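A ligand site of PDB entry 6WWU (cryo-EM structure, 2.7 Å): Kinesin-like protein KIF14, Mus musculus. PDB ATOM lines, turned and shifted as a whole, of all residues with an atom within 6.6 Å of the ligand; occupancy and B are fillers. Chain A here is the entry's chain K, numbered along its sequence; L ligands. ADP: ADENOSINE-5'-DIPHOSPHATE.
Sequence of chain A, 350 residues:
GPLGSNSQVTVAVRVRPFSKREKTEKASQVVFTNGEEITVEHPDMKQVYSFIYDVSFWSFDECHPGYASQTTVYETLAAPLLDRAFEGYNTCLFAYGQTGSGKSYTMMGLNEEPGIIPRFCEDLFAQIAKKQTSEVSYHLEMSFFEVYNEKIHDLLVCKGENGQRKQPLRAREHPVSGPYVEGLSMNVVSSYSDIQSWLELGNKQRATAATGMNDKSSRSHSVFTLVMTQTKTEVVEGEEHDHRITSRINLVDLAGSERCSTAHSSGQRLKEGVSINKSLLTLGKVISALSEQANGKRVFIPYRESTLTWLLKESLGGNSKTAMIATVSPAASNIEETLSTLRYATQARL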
ATOM      1  N   ARG A  14      -1.330 -15.706 -18.100  1.00  0.00           N
ATOM      2  CA  ARG A  14      -1.426 -14.275 -17.736  1.00  0.00           C
ATOM      3  C   ARG A  14      -2.052 -13.476 -18.871  1.00  0.00           C
ATOM      4  O   ARG A  14      -1.640 -13.688 -20.024  1.00  0.00           O
ATOM      5  CB  ARG A  14      -0.017 -13.791 -17.432  1.00  0.00           C
ATOM      6  CG  ARG A  14       0.141 -12.281 -17.328  1.00  0.00           C
ATOM      7  CD  ARG A  14       1.592 -12.011 -17.615  1.00  0.00           C
ATOM      8  NE  ARG A  14       2.055 -10.736 -17.156  1.00  0.00           N
ATOM      9  CZ  ARG A  14       2.141 -10.382 -15.891  1.00  0.00           C
ATOM     10  NH1 ARG A  14       2.905  -9.383 -15.528  1.00  0.00           N
ATOM     11  NH2 ARG A  14       1.468 -11.069 -14.990  1.00  0.00           N
ATOM     12  N   VAL A  15      -2.992 -12.576 -18.579  1.00  0.00           N
ATOM     13  CA  VAL A  15      -3.643 -11.757 -19.619  1.00  0.00           C
ATOM     14  C   VAL A  15      -3.034 -10.352 -19.620  1.00  0.00           C
ATOM     15  O   VAL A  15      -3.427  -9.567 -18.777  1.00  0.00           O
ATOM     16  CB  VAL A  15      -5.154 -11.721 -19.389  1.00  0.00           C
ATOM     17  CG1 VAL A  15      -5.820 -10.730 -20.314  1.00  0.00           C
ATOM     18  CG2 VAL A  15      -5.774 -13.100 -19.525  1.00  0.00           C
ATOM     19  N   ARG A  16      -2.136 -10.063 -20.530  1.00  0.00           N
ATOM     20  CA  ARG A  16      -1.511  -8.719 -20.621  1.00  0.00           C
ATOM     21  C   ARG A  16      -2.581  -7.719 -21.062  1.00  0.00           C
ATOM     22  O   ARG A  16      -3.382  -8.095 -21.920  1.00  0.00           O
ATOM     23  CB  ARG A  16      -0.398  -8.770 -21.668  1.00  0.00           C
ATOM     24  CG  ARG A  16      -0.917  -8.797 -23.091  1.00  0.00           C
ATOM     25  CD  ARG A  16      -0.520  -7.533 -23.801  1.00  0.00           C
ATOM     26  NE  ARG A  16      -0.412  -7.716 -25.227  1.00  0.00           N
ATOM     27  CZ  ARG A  16      -1.405  -7.498 -26.078  1.00  0.00           C
ATOM     28  NH1 ARG A  16      -2.505  -6.899 -25.687  1.00  0.00           N
ATOM     29  NH2 ARG A  16      -1.267  -7.894 -27.328  1.00  0.00           N
ATOM     30  N   PRO A  17      -2.556  -6.482 -20.539  1.00  0.00           N
ATOM     31  CA  PRO A  17      -3.517  -5.432 -20.869  1.00  0.00           C
ATOM     32  C   PRO A  17      -3.345  -4.908 -22.292  1.00  0.00           C
ATOM     33  O   PRO A  17      -2.285  -5.028 -22.822  1.00  0.00           O
ATOM     34  CB  PRO A  17      -3.178  -4.310 -19.899  1.00  0.00           C
ATOM     35  CG  PRO A  17      -1.696  -4.339 -19.895  1.00  0.00           C
ATOM     36  CD  PRO A  17      -1.391  -5.823 -19.962  1.00  0.00           C
ATOM     37  N   SER A  19      -2.611  -2.834 -25.617  1.00  0.00           N
ATOM     38  CA  SER A  19      -1.533  -1.903 -26.046  1.00  0.00           C
ATOM     39  C   SER A  19      -2.164  -0.523 -26.278  1.00  0.00           C
ATOM     40  O   SER A  19      -3.400  -0.468 -26.463  1.00  0.00           O
ATOM     41  CB  SER A  19      -0.830  -2.410 -27.287  1.00  0.00           C
ATOM     42  OG  SER A  19       0.082  -3.446 -26.960  1.00  0.00           O
ATOM     43  N   SER A  59      -4.051  -9.485 -15.413  1.00  0.00           N
ATOM     44  CA  SER A  59      -3.335  -8.209 -15.405  1.00  0.00           C
ATOM     45  C   SER A  59      -3.864  -7.313 -16.523  1.00  0.00           C
ATOM     46  O   SER A  59      -3.064  -6.585 -17.120  1.00  0.00           O
ATOM     47  CB  SER A  59      -1.856  -8.448 -15.513  1.00  0.00           C
ATOM     48  OG  SER A  59      -1.255  -7.532 -16.426  1.00  0.00           O
ATOM     49  N   PHE A  60      -5.173  -7.355 -16.778  1.00  0.00           N
ATOM     50  CA  PHE A  60      -5.842  -6.569 -17.852  1.00  0.00           C
ATOM     51  C   PHE A  60      -6.122  -5.137 -17.373  1.00  0.00           C
ATOM     52  O   PHE A  60      -5.832  -4.192 -18.103  1.00  0.00           O
ATOM     53  CB  PHE A  60      -7.163  -7.218 -18.224  1.00  0.00           C
ATOM     54  CG  PHE A  60      -7.943  -6.507 -19.305  1.00  0.00           C
ATOM     55  CD1 PHE A  60      -7.453  -6.366 -20.580  1.00  0.00           C
ATOM     56  CD2 PHE A  60      -9.176  -5.977 -19.012  1.00  0.00           C
ATOM     57  CE1 PHE A  60      -8.182  -5.709 -21.550  1.00  0.00           C
ATOM     58  CE2 PHE A  60      -9.913  -5.309 -19.978  1.00  0.00           C
ATOM     59  CZ  PHE A  60      -9.409  -5.181 -21.241  1.00  0.00           C
ATOM     60  N   GLU A  62      -6.037  -2.341 -13.717  1.00  0.00           N
ATOM     61  CA  GLU A  62      -5.225  -2.156 -12.516  1.00  0.00           C
ATOM     62  C   GLU A  62      -6.130  -1.965 -11.319  1.00  0.00           C
ATOM     63  O   GLU A  62      -5.681  -1.494 -10.266  1.00  0.00           O
ATOM     64  CB  GLU A  62      -4.267  -0.975 -12.671  1.00  0.00           C
ATOM     65  CG  GLU A  62      -3.541  -0.943 -14.013  1.00  0.00           C
ATOM     66  CD  GLU A  62      -2.138  -0.363 -13.928  1.00  0.00           C
ATOM     67  OE1 GLU A  62      -1.356  -0.594 -14.871  1.00  0.00           O
ATOM     68  OE2 GLU A  62      -1.819   0.330 -12.938  1.00  0.00           O
ATOM     69  N   TYR A  67      -5.768  -8.524  -9.067  1.00  0.00           N
ATOM     70  CA  TYR A  67      -4.810  -8.074 -10.058  1.00  0.00           C
ATOM     71  C   TYR A  67      -3.435  -8.667  -9.788  1.00  0.00           C
ATOM     72  O   TYR A  67      -2.910  -8.564  -8.673  1.00  0.00           O
ATOM     73  CB  TYR A  67      -4.733  -6.549 -10.057  1.00  0.00           C
ATOM     74  CG  TYR A  67      -3.640  -5.980 -10.913  1.00  0.00           C
ATOM     75  CD1 TYR A  67      -3.714  -6.041 -12.287  1.00  0.00           C
ATOM     76  CD2 TYR A  67      -2.550  -5.339 -10.339  1.00  0.00           C
ATOM     77  CE1 TYR A  67      -2.720  -5.506 -13.075  1.00  0.00           C
ATOM     78  CE2 TYR A  67      -1.557  -4.804 -11.127  1.00  0.00           C
ATOM     79  CZ  TYR A  67      -1.650  -4.880 -12.494  1.00  0.00           C
ATOM     80  OH  TYR A  67      -0.658  -4.352 -13.288  1.00  0.00           O
ATOM     81  N   ALA A  68      -2.852  -9.296 -10.805  1.00  0.00           N
ATOM     82  CA  ALA A  68      -1.551  -9.936 -10.693  1.00  0.00           C
ATOM     83  C   ALA A  68      -0.495  -9.076 -11.361  1.00  0.00           C
ATOM     84  O   ALA A  68      -0.398  -9.035 -12.591  1.00  0.00           O
ATOM     85  CB  ALA A  68      -1.598 -11.327 -11.326  1.00  0.00           C
ATOM     86  N   GLN A  70       3.820  -7.885 -11.373  1.00  0.00           N
ATOM     87  CA  GLN A  70       5.066  -8.634 -11.478  1.00  0.00           C
ATOM     88  C   GLN A  70       5.503  -9.259 -10.163  1.00  0.00           C
ATOM     89  O   GLN A  70       6.330 -10.171 -10.189  1.00  0.00           O
ATOM     90  CB  GLN A  70       6.190  -7.715 -11.985  1.00  0.00           C
ATOM     91  CG  GLN A  70       5.983  -7.231 -13.407  1.00  0.00           C
ATOM     92  CD  GLN A  70       6.518  -8.191 -14.431  1.00  0.00           C
ATOM     93  OE1 GLN A  70       5.923  -9.238 -14.694  1.00  0.00           O
ATOM     94  NE2 GLN A  70       7.646  -7.839 -15.045  1.00  0.00           N
ATOM     95  N   GLY A  97       4.270 -18.610 -25.451  1.00  0.00           N
ATOM     96  CA  GLY A  97       3.549 -17.439 -25.897  1.00  0.00           C
ATOM     97  C   GLY A  97       4.013 -17.010 -27.264  1.00  0.00           C
ATOM     98  O   GLY A  97       5.092 -17.377 -27.731  1.00  0.00           O
ATOM     99  N   GLN A  98       3.231 -16.140 -27.935  1.00  0.00           N
ATOM    100  CA  GLN A  98       3.465 -15.665 -29.290  1.00  0.00           C
ATOM    101  C   GLN A  98       3.850 -14.200 -29.184  1.00  0.00           C
ATOM    102  O   GLN A  98       3.922 -13.625 -28.094  1.00  0.00           O
ATOM    103  CB  GLN A  98       2.197 -15.923 -30.084  1.00  0.00           C
ATOM    104  CG  GLN A  98       1.787 -17.384 -30.078  1.00  0.00           C
ATOM    105  CD  GLN A  98       1.858 -17.970 -31.461  1.00  0.00           C
ATOM    106  OE1 GLN A  98       2.658 -17.557 -32.284  1.00  0.00           O
ATOM    107  NE2 GLN A  98       1.002 -18.949 -31.727  1.00  0.00           N
ATOM    108  N   THR A  99       4.139 -13.652 -30.295  1.00  0.00           N
ATOM    109  CA  THR A  99       4.564 -12.258 -30.353  1.00  0.00           C
ATOM    110  C   THR A  99       3.433 -11.335 -29.923  1.00  0.00           C
ATOM    111  O   THR A  99       2.319 -11.411 -30.444  1.00  0.00           O
ATOM    112  CB  THR A  99       5.023 -11.917 -31.773  1.00  0.00           C
ATOM    113  OG1 THR A  99       6.061 -12.824 -32.163  1.00  0.00           O
ATOM    114  CG2 THR A  99       5.525 -10.482 -31.839  1.00  0.00           C
ATOM    115  N   GLY A 100       3.733 -10.456 -28.972  1.00  0.00           N
ATOM    116  CA  GLY A 100       2.764  -9.553 -28.410  1.00  0.00           C
ATOM    117  C   GLY A 100       2.027 -10.067 -27.191  1.00  0.00           C
ATOM    118  O   GLY A 100       1.081  -9.420 -26.745  1.00  0.00           O
ATOM    119  N   SER A 101       2.418 -11.216 -26.643  1.00  0.00           N
ATOM    120  CA  SER A 101       1.689 -11.862 -25.569  1.00  0.00           C
ATOM    121  C   SER A 101       2.112 -11.401 -24.186  1.00  0.00           C
ATOM    122  O   SER A 101       1.295 -11.453 -23.262  1.00  0.00           O
ATOM    123  CB  SER A 101       1.843 -13.380 -25.678  1.00  0.00           C
ATOM    124  OG  SER A 101       3.104 -13.807 -25.178  1.00  0.00           O
ATOM    125  N   GLY A 102       3.361 -10.969 -24.023  1.00  0.00           N
ATOM    126  CA  GLY A 102       3.855 -10.525 -22.734  1.00  0.00           C
ATOM    127  C   GLY A 102       4.842 -11.497 -22.129  1.00  0.00           C
ATOM    128  O   GLY A 102       4.878 -11.696 -20.911  1.00  0.00           O
ATOM    129  N   LYS A 103       5.667 -12.102 -22.979  1.00  0.00           N
ATOM    130  CA  LYS A 103       6.679 -13.051 -22.533  1.00  0.00           C
ATOM    131  C   LYS A 103       7.872 -12.367 -21.883  1.00  0.00           C
ATOM    132  O   LYS A 103       8.247 -12.734 -20.756  1.00  0.00           O
ATOM    133  CB  LYS A 103       7.166 -13.883 -23.723  1.00  0.00           C
ATOM    134  CG  LYS A 103       7.318 -15.354 -23.448  1.00  0.00           C
ATOM    135  CD  LYS A 103       7.985 -16.050 -24.614  1.00  0.00           C
ATOM    136  CE  LYS A 103       7.042 -16.186 -25.787  1.00  0.00           C
ATOM    137  NZ  LYS A 103       7.673 -16.870 -26.924  1.00  0.00           N
ATOM    138  N   SER A 104       8.475 -11.394 -22.550  1.00  0.00           N
ATOM    139  CA  SER A 104       9.625 -10.677 -22.035  1.00  0.00           C
ATOM    140  C   SER A 104       9.277  -9.756 -20.880  1.00  0.00           C
ATOM    141  O   SER A 104      10.119  -9.547 -19.996  1.00  0.00           O
ATOM    142  CB  SER A 104      10.274  -9.862 -23.156  1.00  0.00           C
ATOM    143  OG  SER A 104      11.167  -8.888 -22.629  1.00  0.00           O
ATOM    144  N   TYR A 105       8.073  -9.198 -20.847  1.00  0.00           N
ATOM    145  CA  TYR A 105       7.647  -8.407 -19.706  1.00  0.00           C
ATOM    146  C   TYR A 105       7.478  -9.268 -18.470  1.00  0.00           C
ATOM    147  O   TYR A 105       7.587  -8.763 -17.341  1.00  0.00           O
ATOM    148  CB  TYR A 105       6.331  -7.703 -20.012  1.00  0.00           C
ATOM    149  CG  TYR A 105       5.926  -6.671 -18.970  1.00  0.00           C
ATOM    150  CD1 TYR A 105       5.130  -7.019 -17.896  1.00  0.00           C
ATOM    151  CD2 TYR A 105       6.338  -5.361 -19.084  1.00  0.00           C
ATOM    152  CE1 TYR A 105       4.765  -6.099 -16.953  1.00  0.00           C
ATOM    153  CE2 TYR A 105       5.980  -4.420 -18.136  1.00  0.00           C
ATOM    154  CZ  TYR A 105       5.188  -4.795 -17.078  1.00  0.00           C
ATOM    155  OH  TYR A 105       4.818  -3.866 -16.145  1.00  0.00           O
ATOM    156  N   THR A 106       7.215 -10.553 -18.648  1.00  0.00           N
ATOM    157  CA  THR A 106       6.927 -11.437 -17.522  1.00  0.00           C
ATOM    158  C   THR A 106       8.199 -12.114 -17.031  1.00  0.00           C
ATOM    159  O   THR A 106       8.398 -12.280 -15.819  1.00  0.00           O
ATOM    160  CB  THR A 106       5.896 -12.477 -17.930  1.00  0.00           C
ATOM    161  OG1 THR A 106       4.700 -11.825 -18.368  1.00  0.00           O
ATOM    162  CG2 THR A 106       5.574 -13.398 -16.782  1.00  0.00           C
ATOM    163  N   LEU A 110      10.852  -4.799 -17.783  1.00  0.00           N
ATOM    164  CA  LEU A 110      11.391  -3.495 -18.113  1.00  0.00           C
ATOM    165  C   LEU A 110      12.337  -3.059 -16.994  1.00  0.00           C
ATOM    166  O   LEU A 110      12.561  -3.790 -16.024  1.00  0.00           O
ATOM    167  CB  LEU A 110      10.234  -2.525 -18.340  1.00  0.00           C
ATOM    168  CG  LEU A 110       9.246  -2.892 -19.433  1.00  0.00           C
ATOM    169  CD1 LEU A 110       8.094  -1.912 -19.421  1.00  0.00           C
ATOM    170  CD2 LEU A 110       9.913  -2.904 -20.799  1.00  0.00           C
ATOM    171  N   ASN A 214       5.205  -9.740 -37.178  1.00  0.00           N
ATOM    172  CA  ASN A 214       6.232  -8.827 -36.714  1.00  0.00           C
ATOM    173  C   ASN A 214       7.589  -9.270 -37.268  1.00  0.00           C
ATOM    174  O   ASN A 214       7.866 -10.464 -37.414  1.00  0.00           O
ATOM    175  CB  ASN A 214       6.263  -8.780 -35.186  1.00  0.00           C
ATOM    176  CG  ASN A 214       7.214  -7.723 -34.648  1.00  0.00           C
ATOM    177  OD1 ASN A 214       7.841  -6.988 -35.404  1.00  0.00           O
ATOM    178  ND2 ASN A 214       7.329  -7.646 -33.321  1.00  0.00           N
ATOM    179  N   THR A 327       1.473 -17.017 -21.971  1.00  0.00           N
ATOM    180  CA  THR A 327       0.988 -15.663 -22.153  1.00  0.00           C
ATOM    181  C   THR A 327       0.017 -15.590 -23.326  1.00  0.00           C
ATOM    182  O   THR A 327       0.218 -16.213 -24.378  1.00  0.00           O
ATOM    183  CB  THR A 327       2.150 -14.709 -22.369  1.00  0.00           C
ATOM    184  OG1 THR A 327       2.971 -15.174 -23.458  1.00  0.00           O
ATOM    185  CG2 THR A 327       2.981 -14.632 -21.126  1.00  0.00           C
HETATM  186  PB  ADP L   1       6.976 -10.058 -26.704  1.00  0.00           P
HETATM  187  O1B ADP L   1       8.385  -9.854 -26.277  1.00  0.00           O
HETATM  188  O2B ADP L   1       6.602  -9.257 -27.899  1.00  0.00           O
HETATM  189  O3B ADP L   1       6.555 -11.492 -26.740  1.00  0.00           O
HETATM  190  PA  ADP L   1       6.484  -7.884 -25.230  1.00  0.00           P
HETATM  191  O1A ADP L   1       6.761  -7.770 -23.759  1.00  0.00           O
HETATM  192  O2A ADP L   1       7.502  -7.454 -26.230  1.00  0.00           O
HETATM  193  O3A ADP L   1       6.138  -9.399 -25.553  1.00  0.00           O
HETATM  194  O5' ADP L   1       5.147  -7.071 -25.470  1.00  0.00           O
HETATM  195  C5' ADP L   1       5.245  -5.717 -25.837  1.00  0.00           C
HETATM  196  C4' ADP L   1       4.635  -4.806 -24.782  1.00  0.00           C
HETATM  197  O4' ADP L   1       3.662  -5.468 -23.993  1.00  0.00           O
HETATM  198  C3' ADP L   1       5.644  -4.253 -23.801  1.00  0.00           C
HETATM  199  O3' ADP L   1       6.050  -2.954 -24.196  1.00  0.00           O
HETATM  200  C2' ADP L   1       4.935  -4.254 -22.468  1.00  0.00           C
HETATM  201  O2' ADP L   1       4.818  -2.968 -21.868  1.00  0.00           O
HETATM  202  C1' ADP L   1       3.546  -4.749 -22.782  1.00  0.00           C
HETATM  203  N9  ADP L   1       3.035  -5.609 -21.711  1.00  0.00           N
HETATM  204  C8  ADP L   1       2.908  -6.931 -21.730  1.00  0.00           C
HETATM  205  N7  ADP L   1       2.386  -7.371 -20.567  1.00  0.00           N
HETATM  206  C5  ADP L   1       2.171  -6.317 -19.809  1.00  0.00           C
HETATM  207  C6  ADP L   1       1.637  -6.080 -18.476  1.00  0.00           C
HETATM  208  N6  ADP L   1       1.210  -7.081 -17.703  1.00  0.00           N
HETATM  209  N1  ADP L   1       1.569  -4.822 -18.045  1.00  0.00           N
HETATM  210  C2  ADP L   1       1.980  -3.795 -18.795  1.00  0.00           C
HETATM  211  N3  ADP L   1       2.480  -3.953 -20.022  1.00  0.00           N
HETATM  212  C4  ADP L   1       2.585  -5.158 -20.558  1.00  0.00           C
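A nitrogen (N6) of the ligand is in hydrogen-bond range of the side-chain hydroxyl (OG) of Ser 59 (2.8 Å).
The backbone NH of Gly 100 lies within hydrogen-bond range of an oxygen (O2B) of the ligand, 3.3 Å away.
The backbone NH (N) of Tyr 105 sits at hydrogen-bond distance from an oxygen (O1A) of the ligand (3.5 Å).
The backbone carbonyl oxygen (O) of Val 15 lies close to the backbone NH (N) of Ser 59 (3.4 Å).
The backbone carbonyl oxygen (O) of Gly 100 sits at hydrogen-bond distance from the guanidinium group (NE) of Arg 16, 2.7 Å away.
NE2 of Gln 70 is in hydrogen-bond range of O of Tyr 105 (2.5 Å).
O of Gly 102 sits at hydrogen-bond distance from OG1 of Thr 106, 2.6 Å away.
NE of Arg 14 sits at hydrogen-bond distance from OG1 of Thr 106 (3.1 Å).
The side-chain amide oxygen of Gln 70 sits at hydrogen-bond distance from the guanidinium group of Arg 14 (3.1 Å).
OG of Ser 101 lies within hydrogen-bond range of O of Gln 98, at 3.0 Å.
The side-chain amino group (NZ) of Lys 103 lies within hydrogen-bond range of the backbone carbonyl oxygen (O) of Gly 97, 2.8 Å away.
NH1 of Arg 14 touches N6 of the ligand, 3.6 Å away.
CB of Arg 16 touches N7 of the ligand, at 3.3 Å.
Pro 17 touches the ligand (CD to C6, 3.4 Å).
Gln 98 touches the ligand (O to O3B, 3.6 Å).
N of Gly 102 touches O3A of the ligand, 3.5 Å away.
N of Lys 103 touches O3A of the ligand, 3.8 Å away.
Ser 104 touches the ligand.
Of the 24 residues printed, 10 come within 4 Å of the ligand.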
